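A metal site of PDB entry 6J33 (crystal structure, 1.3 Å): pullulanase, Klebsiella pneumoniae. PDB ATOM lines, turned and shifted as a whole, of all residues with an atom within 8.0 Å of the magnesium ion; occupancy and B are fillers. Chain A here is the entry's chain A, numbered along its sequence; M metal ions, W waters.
The side-chain amide oxygen (OE1) of Gln 1040 lies close to the backbone carbonyl oxygen (O) of Ser 974, at 3.5 Å.
The backbone carbonyl oxygen (O) of Arg 975 is in hydrogen-bond range of the backbone NH (N) of Gln 1040 (2.7 Å).
The side-chain carboxylate (OD2) of Asp 973 is in salt-bridge range of the guanidinium group (NH1) of Arg 975 (2.7 Å).
The side-chain hydroxyl (OG) of Ser 929 lies within hydrogen-bond range of the side-chain carboxylate (OD2) of Asp 973 (2.7 Å).
The backbone NH of Asp 964 lies within hydrogen-bond range of the backbone carbonyl oxygen of Asp 977 (2.9 Å).
The side-chain carboxylate (OD1) of Asp 964 sits at hydrogen-bond distance from the backbone NH (N) of Leu 972.
O of Asp 964 lies within hydrogen-bond range of NE2 of Gln 1044, 2.9 Å away.
OD1 of Asp 964 lies within salt-bridge range of NH1 of Arg 943, 2.9 Å away.
Five residues have an atom within 4 Å of the magnesium ion: Asp 964, Ser 971, Asp 973, Val 976 and Gln 1040.
The magnesium ion is bound by OE1 of Gln 1040 (2.0 Å), O of Asp 973 (2.0 Å), OD2 of Asp 964 (2.1 Å), water W1 (2.1 Å), O of Val 976 (2.1 Å) and OG of Ser 971 (2.2 Å).
Water W1 bridges O of Asp 964 (2.6 Å) and OD1 of Asp 977 (2.7 Å).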
ATOM      1  N   SER A 929      30.382  -7.648  36.259  1.00  0.00           N
ATOM      2  CA  SER A 929      29.472  -6.569  35.914  1.00  0.00           C
ATOM      3  C   SER A 929      28.814  -6.075  37.194  1.00  0.00           C
ATOM      4  O   SER A 929      28.461  -6.897  38.050  1.00  0.00           O
ATOM      5  CB  SER A 929      28.383  -7.050  34.961  1.00  0.00           C
ATOM      6  OG  SER A 929      27.449  -6.013  34.713  1.00  0.00           O
ATOM      7  N   LEU A 931      25.895  -5.358  37.272  1.00  0.00           N
ATOM      8  CA  LEU A 931      24.506  -5.792  37.155  1.00  0.00           C
ATOM      9  C   LEU A 931      24.189  -7.019  38.002  1.00  0.00           C
ATOM     10  O   LEU A 931      23.022  -7.230  38.327  1.00  0.00           O
ATOM     11  CB  LEU A 931      24.182  -6.079  35.687  1.00  0.00           C
ATOM     12  CG  LEU A 931      24.196  -4.839  34.776  1.00  0.00           C
ATOM     13  CD1 LEU A 931      24.074  -5.256  33.323  1.00  0.00           C
ATOM     14  CD2 LEU A 931      23.068  -3.906  35.158  1.00  0.00           C
ATOM     15  N   ARG A 943      14.977  -4.105  37.164  1.00  0.00           N
ATOM     16  CA  ARG A 943      15.875  -4.654  36.191  1.00  0.00           C
ATOM     17  C   ARG A 943      15.926  -6.167  35.990  1.00  0.00           C
ATOM     18  O   ARG A 943      16.297  -6.602  34.942  1.00  0.00           O
ATOM     19  CB  ARG A 943      17.294  -4.191  36.507  1.00  0.00           C
ATOM     20  CG  ARG A 943      17.521  -2.693  36.430  1.00  0.00           C
ATOM     21  CD  ARG A 943      18.890  -2.277  36.903  1.00  0.00           C
ATOM     22  NE  ARG A 943      19.076  -0.836  36.819  1.00  0.00           N
ATOM     23  CZ  ARG A 943      19.815  -0.220  35.918  1.00  0.00           C
ATOM     24  NH1 ARG A 943      20.387  -0.869  34.948  1.00  0.00           N
ATOM     25  NH2 ARG A 943      19.932   1.072  35.964  1.00  0.00           N
ATOM     26  N   ASP A 963      18.440  -6.038  33.161  1.00  0.00           N
ATOM     27  CA  ASP A 963      18.330  -4.945  32.204  1.00  0.00           C
ATOM     28  C   ASP A 963      19.336  -3.839  32.510  1.00  0.00           C
ATOM     29  O   ASP A 963      19.481  -3.407  33.653  1.00  0.00           O
ATOM     30  CB  ASP A 963      16.915  -4.387  32.237  1.00  0.00           C
ATOM     31  CG  ASP A 963      16.629  -3.413  31.101  1.00  0.00           C
ATOM     32  OD1 ASP A 963      17.365  -3.427  30.082  1.00  0.00           O
ATOM     33  OD2 ASP A 963      15.662  -2.638  31.236  1.00  0.00           O
ATOM     34  N   ASP A 964      20.034  -3.381  31.462  1.00  0.00           N
ATOM     35  CA  ASP A 964      20.768  -2.130  31.516  1.00  0.00           C
ATOM     36  C   ASP A 964      20.289  -1.130  30.473  1.00  0.00           C
ATOM     37  O   ASP A 964      20.972  -0.129  30.210  1.00  0.00           O
ATOM     38  CB  ASP A 964      22.282  -2.361  31.391  1.00  0.00           C
ATOM     39  CG  ASP A 964      23.097  -1.303  32.138  1.00  0.00           C
ATOM     40  OD1 ASP A 964      22.644  -0.813  33.192  1.00  0.00           O
ATOM     41  OD2 ASP A 964      24.200  -0.976  31.643  1.00  0.00           O
ATOM     42  N   GLY A 965      19.122  -1.370  29.863  1.00  0.00           N
ATOM     43  CA  GLY A 965      18.628  -0.524  28.806  1.00  0.00           C
ATOM     44  C   GLY A 965      17.885   0.707  29.307  1.00  0.00           C
ATOM     45  O   GLY A 965      17.747   0.953  30.506  1.00  0.00           O
ATOM     46  N   ALA A 970      19.575   4.592  34.223  1.00  0.00           N
ATOM     47  CA  ALA A 970      20.917   4.815  33.720  1.00  0.00           C
ATOM     48  C   ALA A 970      21.580   3.492  33.375  1.00  0.00           C
ATOM     49  O   ALA A 970      21.234   2.431  33.915  1.00  0.00           O
ATOM     50  CB  ALA A 970      21.762   5.548  34.763  1.00  0.00           C
ATOM     51  N   SER A 971      22.523   3.544  32.442  1.00  0.00           N
ATOM     52  CA  SER A 971      23.404   2.416  32.212  1.00  0.00           C
ATOM     53  C   SER A 971      24.354   2.303  33.392  1.00  0.00           C
ATOM     54  O   SER A 971      25.094   3.238  33.687  1.00  0.00           O
ATOM     55  CB  SER A 971      24.200   2.638  30.922  1.00  0.00           C
ATOM     56  OG  SER A 971      25.210   1.656  30.769  1.00  0.00           O
ATOM     57  N   LEU A 972      24.305   1.162  34.085  1.00  0.00           N
ATOM     58  CA  LEU A 972      25.231   0.901  35.176  1.00  0.00           C
ATOM     59  C   LEU A 972      26.476   0.160  34.715  1.00  0.00           C
ATOM     60  O   LEU A 972      27.451   0.085  35.479  1.00  0.00           O
ATOM     61  CB  LEU A 972      24.546   0.097  36.282  1.00  0.00           C
ATOM     62  CG  LEU A 972      23.285   0.712  36.854  1.00  0.00           C
ATOM     63  CD1 LEU A 972      22.605  -0.264  37.799  1.00  0.00           C
ATOM     64  CD2 LEU A 972      23.616   2.013  37.571  1.00  0.00           C
ATOM     65  N   ASP A 973      26.475  -0.382  33.502  1.00  0.00           N
ATOM     66  CA  ASP A 973      27.616  -1.071  32.923  1.00  0.00           C
ATOM     67  C   ASP A 973      27.804  -0.523  31.516  1.00  0.00           C
ATOM     68  O   ASP A 973      26.945  -0.704  30.653  1.00  0.00           O
ATOM     69  CB  ASP A 973      27.370  -2.582  32.873  1.00  0.00           C
ATOM     70  CG  ASP A 973      28.605  -3.373  32.444  1.00  0.00           C
ATOM     71  OD1 ASP A 973      29.401  -2.864  31.623  1.00  0.00           O
ATOM     72  OD2 ASP A 973      28.785  -4.503  32.941  1.00  0.00           O
ATOM     73  N   SER A 974      28.943   0.129  31.284  1.00  0.00           N
ATOM     74  CA  SER A 974      29.183   0.779  30.001  1.00  0.00           C
ATOM     75  C   SER A 974      29.431  -0.217  28.872  1.00  0.00           C
ATOM     76  O   SER A 974      29.381   0.172  27.701  1.00  0.00           O
ATOM     77  CB  SER A 974      30.379   1.732  30.113  1.00  0.00           C
ATOM     78  OG  SER A 974      31.556   1.023  30.429  1.00  0.00           O
ATOM     79  N   ARG A 975      29.712  -1.481  29.188  1.00  0.00           N
ATOM     80  CA  ARG A 975      29.992  -2.477  28.156  1.00  0.00           C
ATOM     81  C   ARG A 975      28.745  -3.151  27.615  1.00  0.00           C
ATOM     82  O   ARG A 975      28.750  -3.613  26.472  1.00  0.00           O
ATOM     83  CB  ARG A 975      30.908  -3.578  28.706  1.00  0.00           C
ATOM     84  CG  ARG A 975      32.190  -3.107  29.347  1.00  0.00           C
ATOM     85  CD  ARG A 975      32.836  -4.259  30.117  1.00  0.00           C
ATOM     86  NE  ARG A 975      31.930  -4.800  31.127  1.00  0.00           N
ATOM     87  CZ  ARG A 975      31.326  -5.979  31.053  1.00  0.00           C
ATOM     88  NH1 ARG A 975      30.522  -6.361  32.039  1.00  0.00           N
ATOM     89  NH2 ARG A 975      31.519  -6.781  30.018  1.00  0.00           N
ATOM     90  N   VAL A 976      27.687  -3.240  28.408  1.00  0.00           N
ATOM     91  CA  VAL A 976      26.516  -4.036  28.053  1.00  0.00           C
ATOM     92  C   VAL A 976      25.223  -3.252  28.274  1.00  0.00           C
ATOM     93  O   VAL A 976      25.137  -2.380  29.141  1.00  0.00           O
ATOM     94  CB  VAL A 976      26.453  -5.375  28.827  1.00  0.00           C
ATOM     95  CG1 VAL A 976      27.722  -6.199  28.599  1.00  0.00           C
ATOM     96  CG2 VAL A 976      26.216  -5.146  30.310  1.00  0.00           C
ATOM     97  N   ASP A 977      24.212  -3.594  27.473  1.00  0.00           N
ATOM     98  CA  ASP A 977      22.843  -3.146  27.672  1.00  0.00           C
ATOM     99  C   ASP A 977      22.005  -4.159  28.444  1.00  0.00           C
ATOM    100  O   ASP A 977      20.829  -3.887  28.734  1.00  0.00           O
ATOM    101  CB  ASP A 977      22.176  -2.845  26.332  1.00  0.00           C
ATOM    102  CG  ASP A 977      22.745  -1.600  25.655  1.00  0.00           C
ATOM    103  OD1 ASP A 977      22.970  -0.592  26.351  1.00  0.00           O
ATOM    104  OD2 ASP A 977      22.939  -1.640  24.431  1.00  0.00           O
ATOM    105  N   GLY A 978      22.558  -5.322  28.751  1.00  0.00           N
ATOM    106  CA  GLY A 978      21.831  -6.314  29.517  1.00  0.00           C
ATOM    107  C   GLY A 978      22.627  -7.596  29.598  1.00  0.00           C
ATOM    108  O   GLY A 978      23.569  -7.811  28.825  1.00  0.00           O
ATOM    109  N   LEU A1038      24.439  -8.380  26.050  1.00  0.00           N
ATOM    110  CA  LEU A1038      24.066  -7.516  24.937  1.00  0.00           C
ATOM    111  C   LEU A1038      25.109  -6.397  24.891  1.00  0.00           C
ATOM    112  O   LEU A1038      25.100  -5.528  25.762  1.00  0.00           O
ATOM    113  CB  LEU A1038      22.685  -6.915  25.165  1.00  0.00           C
ATOM    114  CG  LEU A1038      21.431  -7.767  25.008  1.00  0.00           C
ATOM    115  CD1 LEU A1038      20.206  -6.926  25.324  1.00  0.00           C
ATOM    116  CD2 LEU A1038      21.328  -8.321  23.590  1.00  0.00           C
ATOM    117  N   PRO A1039      26.004  -6.388  23.908  1.00  0.00           N
ATOM    118  CA  PRO A1039      27.068  -5.374  23.904  1.00  0.00           C
ATOM    119  C   PRO A1039      26.492  -3.986  23.705  1.00  0.00           C
ATOM    120  O   PRO A1039      25.552  -3.788  22.924  1.00  0.00           O
ATOM    121  CB  PRO A1039      27.950  -5.785  22.711  1.00  0.00           C
ATOM    122  CG  PRO A1039      27.509  -7.146  22.333  1.00  0.00           C
ATOM    123  CD  PRO A1039      26.091  -7.290  22.745  1.00  0.00           C
ATOM    124  N   GLN A1040      27.052  -3.017  24.416  1.00  0.00           N
ATOM    125  CA  GLN A1040      26.563  -1.658  24.366  1.00  0.00           C
ATOM    126  C   GLN A1040      27.277  -0.907  23.249  1.00  0.00           C
ATOM    127  O   GLN A1040      28.512  -0.934  23.158  1.00  0.00           O
ATOM    128  CB  GLN A1040      26.777  -0.946  25.711  1.00  0.00           C
ATOM    129  CG  GLN A1040      26.118   0.420  25.800  1.00  0.00           C
ATOM    130  CD  GLN A1040      26.080   0.955  27.217  1.00  0.00           C
ATOM    131  OE1 GLN A1040      25.939   0.187  28.181  1.00  0.00           O
ATOM    132  NE2 GLN A1040      26.202   2.268  27.374  1.00  0.00           N
ATOM    133  N   GLY A1041      26.490  -0.267  22.382  1.00  0.00           N
ATOM    134  CA  GLY A1041      27.034   0.465  21.257  1.00  0.00           C
ATOM    135  C   GLY A1041      27.423   1.900  21.578  1.00  0.00           C
ATOM    136  O   GLY A1041      27.922   2.179  22.664  1.00  0.00           O
ATOM    137  N   SER A1043      25.531   4.473  22.117  1.00  0.00           N
ATOM    138  CA  SER A1043      24.699   4.981  23.194  1.00  0.00           C
ATOM    139  C   SER A1043      23.957   3.827  23.834  1.00  0.00           C
ATOM    140  O   SER A1043      23.905   2.714  23.291  1.00  0.00           O
ATOM    141  CB  SER A1043      23.716   6.051  22.696  1.00  0.00           C
ATOM    142  OG  SER A1043      24.398   7.171  22.161  1.00  0.00           O
ATOM    143  N   GLN A1044      23.384   4.085  25.018  1.00  0.00           N
ATOM    144  CA  GLN A1044      22.640   3.070  25.739  1.00  0.00           C
ATOM    145  C   GLN A1044      21.501   2.539  24.875  1.00  0.00           C
ATOM    146  O   GLN A1044      20.788   3.320  24.218  1.00  0.00           O
ATOM    147  CB  GLN A1044      22.067   3.660  27.022  1.00  0.00           C
ATOM    148  CG  GLN A1044      21.132   2.739  27.805  1.00  0.00           C
ATOM    149  CD  GLN A1044      20.502   3.435  29.008  1.00  0.00           C
ATOM    150  OE1 GLN A1044      20.195   4.626  28.952  1.00  0.00           O
ATOM    151  NE2 GLN A1044      20.307   2.697  30.091  1.00  0.00           N
ATOM    152  N   GLY A1045      21.331   1.213  24.860  1.00  0.00           N
ATOM    153  CA  GLY A1045      20.401   0.556  23.983  1.00  0.00           C
ATOM    154  C   GLY A1045      19.101   0.157  24.660  1.00  0.00           C
ATOM    155  O   GLY A1045      18.784   0.571  25.784  1.00  0.00           O
HETATM  156 MG    MG M   1      25.115  -0.373  29.868  1.00  0.00          MG
HETATM  157  O   HOH W   1      23.279   0.049  28.930  1.00  0.00           O
